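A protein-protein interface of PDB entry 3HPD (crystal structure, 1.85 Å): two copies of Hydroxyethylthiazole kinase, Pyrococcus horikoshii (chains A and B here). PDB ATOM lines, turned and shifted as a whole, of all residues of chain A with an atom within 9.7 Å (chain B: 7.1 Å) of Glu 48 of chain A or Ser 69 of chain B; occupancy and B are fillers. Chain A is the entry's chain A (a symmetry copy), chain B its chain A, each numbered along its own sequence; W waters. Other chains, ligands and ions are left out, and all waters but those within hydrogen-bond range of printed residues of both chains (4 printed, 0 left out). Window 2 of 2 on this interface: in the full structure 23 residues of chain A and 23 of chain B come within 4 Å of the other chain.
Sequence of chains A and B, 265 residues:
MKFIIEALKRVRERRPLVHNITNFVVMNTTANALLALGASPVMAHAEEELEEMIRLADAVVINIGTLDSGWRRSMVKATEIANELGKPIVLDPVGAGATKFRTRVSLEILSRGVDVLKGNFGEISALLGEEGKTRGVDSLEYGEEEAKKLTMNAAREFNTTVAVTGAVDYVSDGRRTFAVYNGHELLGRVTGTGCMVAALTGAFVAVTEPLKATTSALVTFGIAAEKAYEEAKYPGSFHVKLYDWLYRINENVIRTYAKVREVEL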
ATOM      1  N   ALA A  44       2.333 -31.453 -22.123  1.00  0.00           N
ATOM      2  CA  ALA A  44       0.985 -30.900 -22.083  1.00  0.00           C
ATOM      3  C   ALA A  44       0.950 -29.729 -21.112  1.00  0.00           C
ATOM      4  O   ALA A  44       1.616 -29.751 -20.074  1.00  0.00           O
ATOM      5  CB  ALA A  44      -0.008 -31.969 -21.654  1.00  0.00           C
ATOM      6  N   HIS A  45       0.163 -28.712 -21.441  1.00  0.00           N
ATOM      7  CA  HIS A  45       0.078 -27.527 -20.597  1.00  0.00           C
ATOM      8  C   HIS A  45      -1.334 -26.959 -20.447  1.00  0.00           C
ATOM      9  O   HIS A  45      -1.586 -26.164 -19.547  1.00  0.00           O
ATOM     10  CB  HIS A  45       0.982 -26.431 -21.167  1.00  0.00           C
ATOM     11  CG  HIS A  45       0.544 -25.938 -22.511  1.00  0.00           C
ATOM     12  ND1 HIS A  45       0.702 -26.678 -23.661  1.00  0.00           N
ATOM     13  CD2 HIS A  45      -0.106 -24.807 -22.875  1.00  0.00           C
ATOM     14  CE1 HIS A  45       0.164 -26.026 -24.680  1.00  0.00           C
ATOM     15  NE2 HIS A  45      -0.333 -24.890 -24.229  1.00  0.00           N
ATOM     16  N   ALA A  46      -2.248 -27.351 -21.330  1.00  0.00           N
ATOM     17  CA  ALA A  46      -3.609 -26.820 -21.276  1.00  0.00           C
ATOM     18  C   ALA A  46      -4.272 -27.051 -19.924  1.00  0.00           C
ATOM     19  O   ALA A  46      -4.318 -28.176 -19.425  1.00  0.00           O
ATOM     20  CB  ALA A  46      -4.462 -27.431 -22.392  1.00  0.00           C
ATOM     21  N   GLU A  47      -4.786 -25.978 -19.331  1.00  0.00           N
ATOM     22  CA  GLU A  47      -5.441 -26.094 -18.036  1.00  0.00           C
ATOM     23  C   GLU A  47      -6.636 -27.038 -18.116  1.00  0.00           C
ATOM     24  O   GLU A  47      -7.042 -27.623 -17.109  1.00  0.00           O
ATOM     25  CB  GLU A  47      -5.863 -24.710 -17.538  1.00  0.00           C
ATOM     26  CG  GLU A  47      -4.695 -23.908 -16.973  1.00  0.00           C
ATOM     27  CD  GLU A  47      -5.044 -22.460 -16.698  1.00  0.00           C
ATOM     28  OE1 GLU A  47      -6.078 -22.206 -16.042  1.00  0.00           O
ATOM     29  OE2 GLU A  47      -4.278 -21.575 -17.133  1.00  0.00           O
ATOM     30  N   GLU A  48      -7.181 -27.204 -19.320  1.00  0.00           N
ATOM     31  CA  GLU A  48      -8.321 -28.089 -19.522  1.00  0.00           C
ATOM     32  C   GLU A  48      -7.987 -29.575 -19.379  1.00  0.00           C
ATOM     33  O   GLU A  48      -8.892 -30.400 -19.281  1.00  0.00           O
ATOM     34  CB  GLU A  48      -8.959 -27.858 -20.896  1.00  0.00           C
ATOM     35  CG  GLU A  48      -9.689 -26.536 -21.032  1.00  0.00           C
ATOM     36  CD  GLU A  48      -8.803 -25.421 -21.552  1.00  0.00           C
ATOM     37  OE1 GLU A  48      -7.568 -25.500 -21.379  1.00  0.00           O
ATOM     38  OE2 GLU A  48      -9.348 -24.454 -22.126  1.00  0.00           O
ATOM     39  N   GLU A  49      -6.701 -29.921 -19.375  1.00  0.00           N
ATOM     40  CA  GLU A  49      -6.311 -31.322 -19.242  1.00  0.00           C
ATOM     41  C   GLU A  49      -5.199 -31.575 -18.226  1.00  0.00           C
ATOM     42  O   GLU A  49      -4.744 -32.707 -18.087  1.00  0.00           O
ATOM     43  CB  GLU A  49      -5.875 -31.888 -20.600  1.00  0.00           C
ATOM     44  CG  GLU A  49      -4.539 -31.354 -21.107  1.00  0.00           C
ATOM     45  CD  GLU A  49      -4.123 -31.971 -22.433  1.00  0.00           C
ATOM     46  OE1 GLU A  49      -4.789 -32.927 -22.888  1.00  0.00           O
ATOM     47  OE2 GLU A  49      -3.123 -31.502 -23.019  1.00  0.00           O
ATOM     48  N   LEU A  50      -4.763 -30.539 -17.512  1.00  0.00           N
ATOM     49  CA  LEU A  50      -3.696 -30.717 -16.529  1.00  0.00           C
ATOM     50  C   LEU A  50      -4.002 -31.785 -15.487  1.00  0.00           C
ATOM     51  O   LEU A  50      -3.161 -32.632 -15.201  1.00  0.00           O
ATOM     52  CB  LEU A  50      -3.388 -29.404 -15.802  1.00  0.00           C
ATOM     53  CG  LEU A  50      -2.611 -28.333 -16.564  1.00  0.00           C
ATOM     54  CD1 LEU A  50      -2.444 -27.100 -15.677  1.00  0.00           C
ATOM     55  CD2 LEU A  50      -1.249 -28.883 -16.975  1.00  0.00           C
ATOM     56  N   GLU A  51      -5.198 -31.752 -14.910  1.00  0.00           N
ATOM     57  CA  GLU A  51      -5.531 -32.740 -13.890  1.00  0.00           C
ATOM     58  C   GLU A  51      -5.465 -34.168 -14.420  1.00  0.00           C
ATOM     59  O   GLU A  51      -4.833 -35.031 -13.811  1.00  0.00           O
ATOM     60  CB  GLU A  51      -6.913 -32.464 -13.290  1.00  0.00           C
ATOM     61  CG  GLU A  51      -7.332 -33.497 -12.247  1.00  0.00           C
ATOM     62  CD  GLU A  51      -8.186 -32.910 -11.136  1.00  0.00           C
ATOM     63  OE1 GLU A  51      -7.688 -32.811  -9.993  1.00  0.00           O
ATOM     64  OE2 GLU A  51      -9.348 -32.542 -11.406  1.00  0.00           O
ATOM     65  N   GLU A  52      -6.100 -34.419 -15.559  1.00  0.00           N
ATOM     66  CA  GLU A  52      -6.095 -35.763 -16.129  1.00  0.00           C
ATOM     67  C   GLU A  52      -4.703 -36.232 -16.539  1.00  0.00           C
ATOM     68  O   GLU A  52      -4.370 -37.408 -16.387  1.00  0.00           O
ATOM     69  CB  GLU A  52      -7.035 -35.829 -17.332  1.00  0.00           C
ATOM     70  CG  GLU A  52      -8.501 -35.723 -16.954  1.00  0.00           C
ATOM     71  CD  GLU A  52      -9.402 -35.579 -18.164  1.00  0.00           C
ATOM     72  OE1 GLU A  52      -9.485 -36.531 -18.961  1.00  0.00           O
ATOM     73  OE2 GLU A  52     -10.020 -34.506 -18.315  1.00  0.00           O
ATOM     74  N   MET A  53      -3.887 -35.316 -17.047  1.00  0.00           N
ATOM     75  CA  MET A  53      -2.542 -35.677 -17.478  1.00  0.00           C
ATOM     76  C   MET A  53      -1.619 -35.958 -16.286  1.00  0.00           C
ATOM     77  O   MET A  53      -0.850 -36.919 -16.304  1.00  0.00           O
ATOM     78  CB  MET A  53      -1.957 -34.566 -18.359  1.00  0.00           C
ATOM     79  CG  MET A  53      -0.878 -35.053 -19.311  1.00  0.00           C
ATOM     80  SD  MET A  53      -1.486 -36.348 -20.421  1.00  0.00           S
ATOM     81  CE  MET A  53      -1.967 -35.386 -21.867  1.00  0.00           C
ATOM     82  N   ILE A  54      -1.702 -35.134 -15.246  1.00  0.00           N
ATOM     83  CA  ILE A  54      -0.862 -35.327 -14.066  1.00  0.00           C
ATOM     84  C   ILE A  54      -1.286 -36.592 -13.316  1.00  0.00           C
ATOM     85  O   ILE A  54      -0.473 -37.242 -12.657  1.00  0.00           O
ATOM     86  CB  ILE A  54      -0.930 -34.098 -13.134  1.00  0.00           C
ATOM     87  CG1 ILE A  54      -0.377 -32.873 -13.874  1.00  0.00           C
ATOM     88  CG2 ILE A  54      -0.107 -34.344 -11.866  1.00  0.00           C
ATOM     89  CD1 ILE A  54      -0.492 -31.578 -13.106  1.00  0.00           C
ATOM     90  N   GLY A  70       0.572 -17.104 -19.515  1.00  0.00           N
ATOM     91  CA  GLY A  70      -0.247 -18.285 -19.722  1.00  0.00           C
ATOM     92  C   GLY A  70       0.404 -19.548 -19.190  1.00  0.00           C
ATOM     93  O   GLY A  70      -0.232 -20.334 -18.485  1.00  0.00           O
ATOM     94  N   ARG A  73       0.599 -19.774 -15.311  1.00  0.00           N
ATOM     95  CA  ARG A  73      -0.655 -20.222 -14.721  1.00  0.00           C
ATOM     96  C   ARG A  73      -0.708 -21.747 -14.738  1.00  0.00           C
ATOM     97  O   ARG A  73      -1.064 -22.378 -13.739  1.00  0.00           O
ATOM     98  CB  ARG A  73      -1.826 -19.643 -15.513  1.00  0.00           C
ATOM     99  CG  ARG A  73      -3.157 -19.663 -14.790  1.00  0.00           C
ATOM    100  CD  ARG A  73      -4.198 -18.898 -15.594  1.00  0.00           C
ATOM    101  NE  ARG A  73      -3.697 -17.584 -15.996  1.00  0.00           N
ATOM    102  CZ  ARG A  73      -3.537 -17.198 -17.259  1.00  0.00           C
ATOM    103  NH1 ARG A  73      -3.841 -18.023 -18.254  1.00  0.00           N
ATOM    104  NH2 ARG A  73      -3.067 -15.987 -17.528  1.00  0.00           N
ATOM    105  N   SER A  74      -0.341 -22.338 -15.872  1.00  0.00           N
ATOM    106  CA  SER A  74      -0.342 -23.790 -16.004  1.00  0.00           C
ATOM    107  C   SER A  74       0.670 -24.449 -15.066  1.00  0.00           C
ATOM    108  O   SER A  74       0.377 -25.467 -14.441  1.00  0.00           O
ATOM    109  CB  SER A  74      -0.038 -24.198 -17.451  1.00  0.00           C
ATOM    110  OG  SER A  74      -1.115 -23.868 -18.319  1.00  0.00           O
ATOM    111  N   LYS A  77      -0.500 -24.197 -11.371  1.00  0.00           N
ATOM    112  CA  LYS A  77      -1.639 -25.088 -11.177  1.00  0.00           C
ATOM    113  C   LYS A  77      -1.161 -26.536 -11.160  1.00  0.00           C
ATOM    114  O   LYS A  77      -1.617 -27.340 -10.347  1.00  0.00           O
ATOM    115  CB  LYS A  77      -2.661 -24.895 -12.299  1.00  0.00           C
ATOM    116  CG  LYS A  77      -3.951 -25.682 -12.113  1.00  0.00           C
ATOM    117  CD  LYS A  77      -4.721 -25.211 -10.884  1.00  0.00           C
ATOM    118  CE  LYS A  77      -5.999 -26.019 -10.687  1.00  0.00           C
ATOM    119  NZ  LYS A  77      -6.744 -25.600  -9.464  1.00  0.00           N
ATOM    120  N   ILE A  81      -1.633 -29.401  -8.284  1.00  0.00           N
ATOM    121  CA  ILE A  81      -2.267 -30.683  -8.591  1.00  0.00           C
ATOM    122  C   ILE A  81      -1.337 -31.849  -8.258  1.00  0.00           C
ATOM    123  O   ILE A  81      -1.742 -32.815  -7.604  1.00  0.00           O
ATOM    124  CB  ILE A  81      -2.654 -30.762 -10.085  1.00  0.00           C
ATOM    125  CG1 ILE A  81      -3.747 -29.735 -10.391  1.00  0.00           C
ATOM    126  CG2 ILE A  81      -3.120 -32.171 -10.436  1.00  0.00           C
ATOM    127  CD1 ILE A  81      -4.094 -29.631 -11.860  1.00  0.00           C
ATOM    128  N   GLU B  47      -5.164 -16.974 -36.315  1.00  0.00           N
ATOM    129  CA  GLU B  47      -6.463 -16.832 -36.957  1.00  0.00           C
ATOM    130  C   GLU B  47      -6.443 -15.697 -37.974  1.00  0.00           C
ATOM    131  O   GLU B  47      -7.236 -15.687 -38.919  1.00  0.00           O
ATOM    132  CB  GLU B  47      -7.547 -16.606 -35.900  1.00  0.00           C
ATOM    133  CG  GLU B  47      -7.944 -17.893 -35.182  1.00  0.00           C
ATOM    134  CD  GLU B  47      -8.833 -17.654 -33.980  1.00  0.00           C
ATOM    135  OE1 GLU B  47      -9.841 -16.925 -34.114  1.00  0.00           O
ATOM    136  OE2 GLU B  47      -8.527 -18.204 -32.901  1.00  0.00           O
ATOM    137  N   LEU B  67      -2.100 -29.173 -27.661  1.00  0.00           N
ATOM    138  CA  LEU B  67      -3.151 -28.173 -27.789  1.00  0.00           C
ATOM    139  C   LEU B  67      -3.539 -27.433 -26.516  1.00  0.00           C
ATOM    140  O   LEU B  67      -3.189 -27.832 -25.407  1.00  0.00           O
ATOM    141  CB  LEU B  67      -4.418 -28.810 -28.376  1.00  0.00           C
ATOM    142  CG  LEU B  67      -5.038 -30.073 -27.753  1.00  0.00           C
ATOM    143  CD1 LEU B  67      -4.592 -30.282 -26.315  1.00  0.00           C
ATOM    144  CD2 LEU B  67      -6.557 -29.965 -27.842  1.00  0.00           C
ATOM    145  N   ASP B  68      -4.247 -26.327 -26.712  1.00  0.00           N
ATOM    146  CA  ASP B  68      -4.796 -25.520 -25.630  1.00  0.00           C
ATOM    147  C   ASP B  68      -6.007 -24.817 -26.243  1.00  0.00           C
ATOM    148  O   ASP B  68      -6.306 -25.031 -27.423  1.00  0.00           O
ATOM    149  CB  ASP B  68      -3.774 -24.526 -25.034  1.00  0.00           C
ATOM    150  CG  ASP B  68      -3.208 -23.545 -26.049  1.00  0.00           C
ATOM    151  OD1 ASP B  68      -3.946 -23.096 -26.948  1.00  0.00           O
ATOM    152  OD2 ASP B  68      -2.012 -23.200 -25.916  1.00  0.00           O
ATOM    153  N   SER B  69      -6.720 -24.008 -25.462  1.00  0.00           N
ATOM    154  CA  SER B  69      -7.911 -23.341 -25.979  1.00  0.00           C
ATOM    155  C   SER B  69      -7.643 -22.498 -27.223  1.00  0.00           C
ATOM    156  O   SER B  69      -8.462 -22.465 -28.144  1.00  0.00           O
ATOM    157  CB  SER B  69      -8.556 -22.474 -24.888  1.00  0.00           C
ATOM    158  OG  SER B  69      -7.667 -21.479 -24.418  1.00  0.00           O
ATOM    159  N   GLY B  70      -6.496 -21.828 -27.250  1.00  0.00           N
ATOM    160  CA  GLY B  70      -6.153 -21.000 -28.393  1.00  0.00           C
ATOM    161  C   GLY B  70      -5.932 -21.809 -29.657  1.00  0.00           C
ATOM    162  O   GLY B  70      -6.466 -21.478 -30.717  1.00  0.00           O
ATOM    163  N   TRP B  71      -5.143 -22.874 -29.558  1.00  0.00           N
ATOM    164  CA  TRP B  71      -4.873 -23.706 -30.723  1.00  0.00           C
ATOM    165  C   TRP B  71      -6.113 -24.463 -31.178  1.00  0.00           C
ATOM    166  O   TRP B  71      -6.287 -24.718 -32.370  1.00  0.00           O
ATOM    167  CB  TRP B  71      -3.728 -24.683 -30.431  1.00  0.00           C
ATOM    168  CG  TRP B  71      -2.394 -24.001 -30.381  1.00  0.00           C
ATOM    169  CD1 TRP B  71      -1.932 -23.170 -29.398  1.00  0.00           C
ATOM    170  CD2 TRP B  71      -1.376 -24.035 -31.387  1.00  0.00           C
ATOM    171  NE1 TRP B  71      -0.690 -22.680 -29.734  1.00  0.00           N
ATOM    172  CE2 TRP B  71      -0.325 -23.195 -30.952  1.00  0.00           C
ATOM    173  CE3 TRP B  71      -1.250 -24.688 -32.620  1.00  0.00           C
ATOM    174  CZ2 TRP B  71       0.839 -22.995 -31.703  1.00  0.00           C
ATOM    175  CZ3 TRP B  71      -0.089 -24.487 -33.370  1.00  0.00           C
ATOM    176  CH2 TRP B  71       0.935 -23.646 -32.907  1.00  0.00           C
ATOM    177  N   ARG B  72      -6.979 -24.817 -30.234  1.00  0.00           N
ATOM    178  CA  ARG B  72      -8.205 -25.537 -30.574  1.00  0.00           C
ATOM    179  C   ARG B  72      -9.043 -24.671 -31.507  1.00  0.00           C
ATOM    180  O   ARG B  72      -9.579 -25.147 -32.507  1.00  0.00           O
ATOM    181  CB  ARG B  72      -9.018 -25.849 -29.317  1.00  0.00           C
ATOM    182  CG  ARG B  72     -10.254 -26.704 -29.591  1.00  0.00           C
ATOM    183  CD  ARG B  72     -11.195 -26.726 -28.394  1.00  0.00           C
ATOM    184  NE  ARG B  72     -11.951 -25.485 -28.292  1.00  0.00           N
ATOM    185  CZ  ARG B  72     -12.987 -25.177 -29.068  1.00  0.00           C
ATOM    186  NH1 ARG B  72     -13.397 -26.029 -29.998  1.00  0.00           N
ATOM    187  NH2 ARG B  72     -13.603 -24.012 -28.924  1.00  0.00           N
ATOM    188  N   ARG B  73      -9.150 -23.394 -31.163  1.00  0.00           N
ATOM    189  CA  ARG B  73      -9.914 -22.442 -31.957  1.00  0.00           C
ATOM    190  C   ARG B  73      -9.355 -22.400 -33.376  1.00  0.00           C
ATOM    191  O   ARG B  73     -10.107 -22.434 -34.354  1.00  0.00           O
ATOM    192  CB  ARG B  73      -9.831 -21.059 -31.314  1.00  0.00           C
ATOM    193  CG  ARG B  73     -10.894 -20.080 -31.766  1.00  0.00           C
ATOM    194  CD  ARG B  73     -10.824 -18.812 -30.927  1.00  0.00           C
ATOM    195  NE  ARG B  73     -10.794 -19.123 -29.499  1.00  0.00           N
ATOM    196  CZ  ARG B  73      -9.787 -18.812 -28.686  1.00  0.00           C
ATOM    197  NH1 ARG B  73      -8.720 -18.176 -29.156  1.00  0.00           N
ATOM    198  NH2 ARG B  73      -9.844 -19.143 -27.403  1.00  0.00           N
ATOM    199  N   SER B  74      -8.030 -22.337 -33.487  1.00  0.00           N
ATOM    200  CA  SER B  74      -7.380 -22.301 -34.792  1.00  0.00           C
ATOM    201  C   SER B  74      -7.614 -23.589 -35.581  1.00  0.00           C
ATOM    202  O   SER B  74      -7.878 -23.550 -36.782  1.00  0.00           O
ATOM    203  CB  SER B  74      -5.873 -22.065 -34.634  1.00  0.00           C
ATOM    204  OG  SER B  74      -5.599 -20.745 -34.183  1.00  0.00           O
ATOM    205  N   THR B  99      -7.059 -37.880 -22.363  1.00  0.00           N
ATOM    206  CA  THR B  99      -7.747 -36.793 -21.671  1.00  0.00           C
ATOM    207  C   THR B  99      -9.024 -36.510 -22.444  1.00  0.00           C
ATOM    208  O   THR B  99      -9.064 -36.682 -23.665  1.00  0.00           O
ATOM    209  CB  THR B  99      -6.906 -35.491 -21.608  1.00  0.00           C
ATOM    210  OG1 THR B  99      -6.798 -34.918 -22.918  1.00  0.00           O
ATOM    211  CG2 THR B  99      -5.512 -35.774 -21.050  1.00  0.00           C
ATOM    212  N   LYS B 100     -10.068 -36.095 -21.734  1.00  0.00           N
ATOM    213  CA  LYS B 100     -11.347 -35.794 -22.365  1.00  0.00           C
ATOM    214  C   LYS B 100     -11.183 -34.638 -23.342  1.00  0.00           C
ATOM    215  O   LYS B 100     -11.820 -34.606 -24.393  1.00  0.00           O
ATOM    216  CB  LYS B 100     -12.389 -35.416 -21.307  1.00  0.00           C
ATOM    217  CG  LYS B 100     -12.698 -36.503 -20.287  1.00  0.00           C
ATOM    218  CD  LYS B 100     -13.650 -35.968 -19.219  1.00  0.00           C
ATOM    219  CE  LYS B 100     -13.901 -36.987 -18.122  1.00  0.00           C
ATOM    220  NZ  LYS B 100     -14.776 -36.431 -17.051  1.00  0.00           N
ATOM    221  N   PHE B 101     -10.329 -33.686 -22.978  1.00  0.00           N
ATOM    222  CA  PHE B 101     -10.064 -32.514 -23.807  1.00  0.00           C
ATOM    223  C   PHE B 101      -9.610 -32.921 -25.208  1.00  0.00           C
ATOM    224  O   PHE B 101     -10.101 -32.394 -26.204  1.00  0.00           O
ATOM    225  CB  PHE B 101      -9.000 -31.637 -23.129  1.00  0.00           C
ATOM    226  CG  PHE B 101      -8.746 -30.321 -23.822  1.00  0.00           C
ATOM    227  CD1 PHE B 101      -9.804 -29.519 -24.243  1.00  0.00           C
ATOM    228  CD2 PHE B 101      -7.442 -29.864 -24.015  1.00  0.00           C
ATOM    229  CE1 PHE B 101      -9.569 -28.279 -24.842  1.00  0.00           C
ATOM    230  CE2 PHE B 101      -7.196 -28.627 -24.610  1.00  0.00           C
ATOM    231  CZ  PHE B 101      -8.261 -27.832 -25.026  1.00  0.00           C
ATOM    232  N   ARG B 102      -8.680 -33.869 -25.283  1.00  0.00           N
ATOM    233  CA  ARG B 102      -8.173 -34.327 -26.572  1.00  0.00           C
ATOM    234  C   ARG B 102      -9.206 -35.140 -27.339  1.00  0.00           C
ATOM    235  O   ARG B 102      -9.312 -35.029 -28.559  1.00  0.00           O
ATOM    236  CB  ARG B 102      -6.894 -35.139 -26.368  1.00  0.00           C
ATOM    237  CG  ARG B 102      -5.799 -34.291 -25.765  1.00  0.00           C
ATOM    238  CD  ARG B 102      -4.524 -35.053 -25.524  1.00  0.00           C
ATOM    239  NE  ARG B 102      -3.529 -34.159 -24.946  1.00  0.00           N
ATOM    240  CZ  ARG B 102      -2.289 -34.030 -25.395  1.00  0.00           C
ATOM    241  NH1 ARG B 102      -1.882 -34.746 -26.436  1.00  0.00           N
ATOM    242  NH2 ARG B 102      -1.462 -33.176 -24.810  1.00  0.00           N
ATOM    243  N   ARG B 104     -12.483 -34.862 -26.963  1.00  0.00           N
ATOM    244  CA  ARG B 104     -13.515 -33.899 -27.337  1.00  0.00           C
ATOM    245  C   ARG B 104     -13.143 -33.092 -28.577  1.00  0.00           C
ATOM    246  O   ARG B 104     -13.935 -32.985 -29.517  1.00  0.00           O
ATOM    247  CB  ARG B 104     -13.803 -32.951 -26.165  1.00  0.00           C
ATOM    248  CG  ARG B 104     -14.732 -31.800 -26.522  1.00  0.00           C
ATOM    249  CD  ARG B 104     -15.230 -31.028 -25.296  1.00  0.00           C
ATOM    250  NE  ARG B 104     -14.165 -30.370 -24.539  1.00  0.00           N
ATOM    251  CZ  ARG B 104     -13.667 -30.826 -23.392  1.00  0.00           C
ATOM    252  NH1 ARG B 104     -14.134 -31.950 -22.865  1.00  0.00           N
ATOM    253  NH2 ARG B 104     -12.713 -30.153 -22.762  1.00  0.00           N
HETATM  254  O   HOH W   1      -1.739 -29.213 -23.494  1.00  0.00           O
HETATM  255  O   HOH W   2      -6.043 -23.683 -22.694  1.00  0.00           O
HETATM  256  O   HOH W   3      -9.359 -33.026 -20.321  1.00  0.00           O
HETATM  257  O   HOH W   4      -8.066 -21.702 -21.329  1.00  0.00           O
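The side-chain carboxylate of Asp 68 of chain B is in hydrogen-bond range of a ring nitrogen (NE2) of His 45 of chain A (2.9 Å).
The side-chain hydroxyl (OG1) of Thr 99 of chain B lies within hydrogen-bond range of the side-chain carboxylate (OE1) of Glu 49 of chain A.
The backbone NH (N) of Lys 100 of chain B lies within hydrogen-bond range of the side-chain carboxylate (OE1) of Glu 52 of chain A, at 2.9 Å.
NE of Arg 102 of chain B is in salt-bridge range of OE1 of Glu 49 of chain A (2.7 Å).
The backbone NH (N) of Gly 70 of chain B sits at hydrogen-bond distance from the side-chain carboxylate (OD1) of Asp 68 of chain B (2.9 Å).
The side-chain carboxylate (OD1) of Asp 68 of chain B is in hydrogen-bond range of the backbone NH (N) of Trp 71 of chain B, 2.9 Å away.
The backbone NH (N) of Arg 102 of chain B sits close to the side-chain hydroxyl (OG1) of Thr 99 of chain B.
The side-chain hydroxyl of Ser 74 of chain A lies within hydrogen-bond range of the backbone carbonyl oxygen of His 45 of chain A (2.6 Å).
Among the printed residues, merely in contact across the chains: Ala 44 of chain A with Arg 102 of chain B (3.7 Å), His 45 of chain A with Leu 67 of chain B (3.9 Å), Ala 46 of chain A with Leu 67 of chain B (3.3 Å), Ala 46 of chain A with Asp 68 of chain B (3.8 Å), Ala 46 of chain A with Phe 101 of chain B (3.7 Å), Glu 48 of chain A with Ser 69 of chain B (3.5 Å), Glu 48 of chain A with Phe 101 of chain B (3.8 Å), Glu 49 of chain A with Leu 67 of chain B (3.8 Å), Glu 52 of chain A with Thr 99 of chain B (3.2 Å), Met 53 of chain A with Thr 99 of chain B (3.7 Å) and Met 53 of chain A with Arg 102 of chain B (3.7 Å).
Printed residues of chain B within 4 Å of His 45 of chain A: Leu 67 (3.9 Å) and Asp 68 (2.9 Å).
Of the printed residues of chain B, Glu 48 of chain A touches Ser 69 and Phe 101.
Of the printed residues of chain B, Glu 52 of chain A touches Thr 99 and Lys 100.
Of chain A, only His 45 (2.9 Å) and Ala 46 (3.8 Å) come within 4 Å of Asp 68 of chain B.
Ser 69 of chain B touches one residue of chain A.
Of the printed residues of chain A, Phe 101 of chain B touches Ala 46 and Glu 48.
The nearest printed residue of chain A that does not touch Thr 99 of chain B is Glu 48 of chain A (5.9 Å).
Of the 14 printed residues of chain B, 7 touch a printed residue of chain A.
Printed residues of chain B that touch a printed residue of chain A: Leu 67, Asp 68, Ser 69, Thr 99, Lys 100, Phe 101 and Arg 102.
Printed residues of chain A that touch a printed residue of chain B: Ala 44, His 45, Ala 46, Glu 48, Glu 49, Glu 52 and Met 53.
Among the printed residues, 15 pairs touch across the chains.
Among the printed residues, Asp or Glu carboxylates within 4 Å of a Lys or Arg side-chain nitrogen of the other chain: Glu 49 of chain A with Arg 102 of chain B (2.7 Å).
Positions printed for both chains: 47, 70, 73 and 74.
Water W3 lies within hydrogen-bond range of OE2 of Glu 52 of chain A (2.6 Å), O of Glu 48 of chain A (2.9 Å), N of Phe 101 of chain B (2.9 Å) and N of Lys 100 of chain B (3.5 Å).
Water W2 bridges the side-chain carboxylate (OE1) of Glu 48 of chain A (2.7 Å) and the backbone NH (N) of Ser 69 of chain B (2.9 Å).
Water W1 lies within hydrogen-bond range of the side-chain carboxylate of Glu 49 of chain A (2.7 Å), the backbone carbonyl oxygen of Leu 67 of chain B (2.8 Å), the backbone NH of His 45 of chain A (2.8 Å) and the backbone NH of Ala 46 of chain A (2.9 Å).
Water W4 bridges the side-chain hydroxyl (OG) of Ser 69 of chain B and the side-chain carboxylate (OE2) of Glu 48 of chain A.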
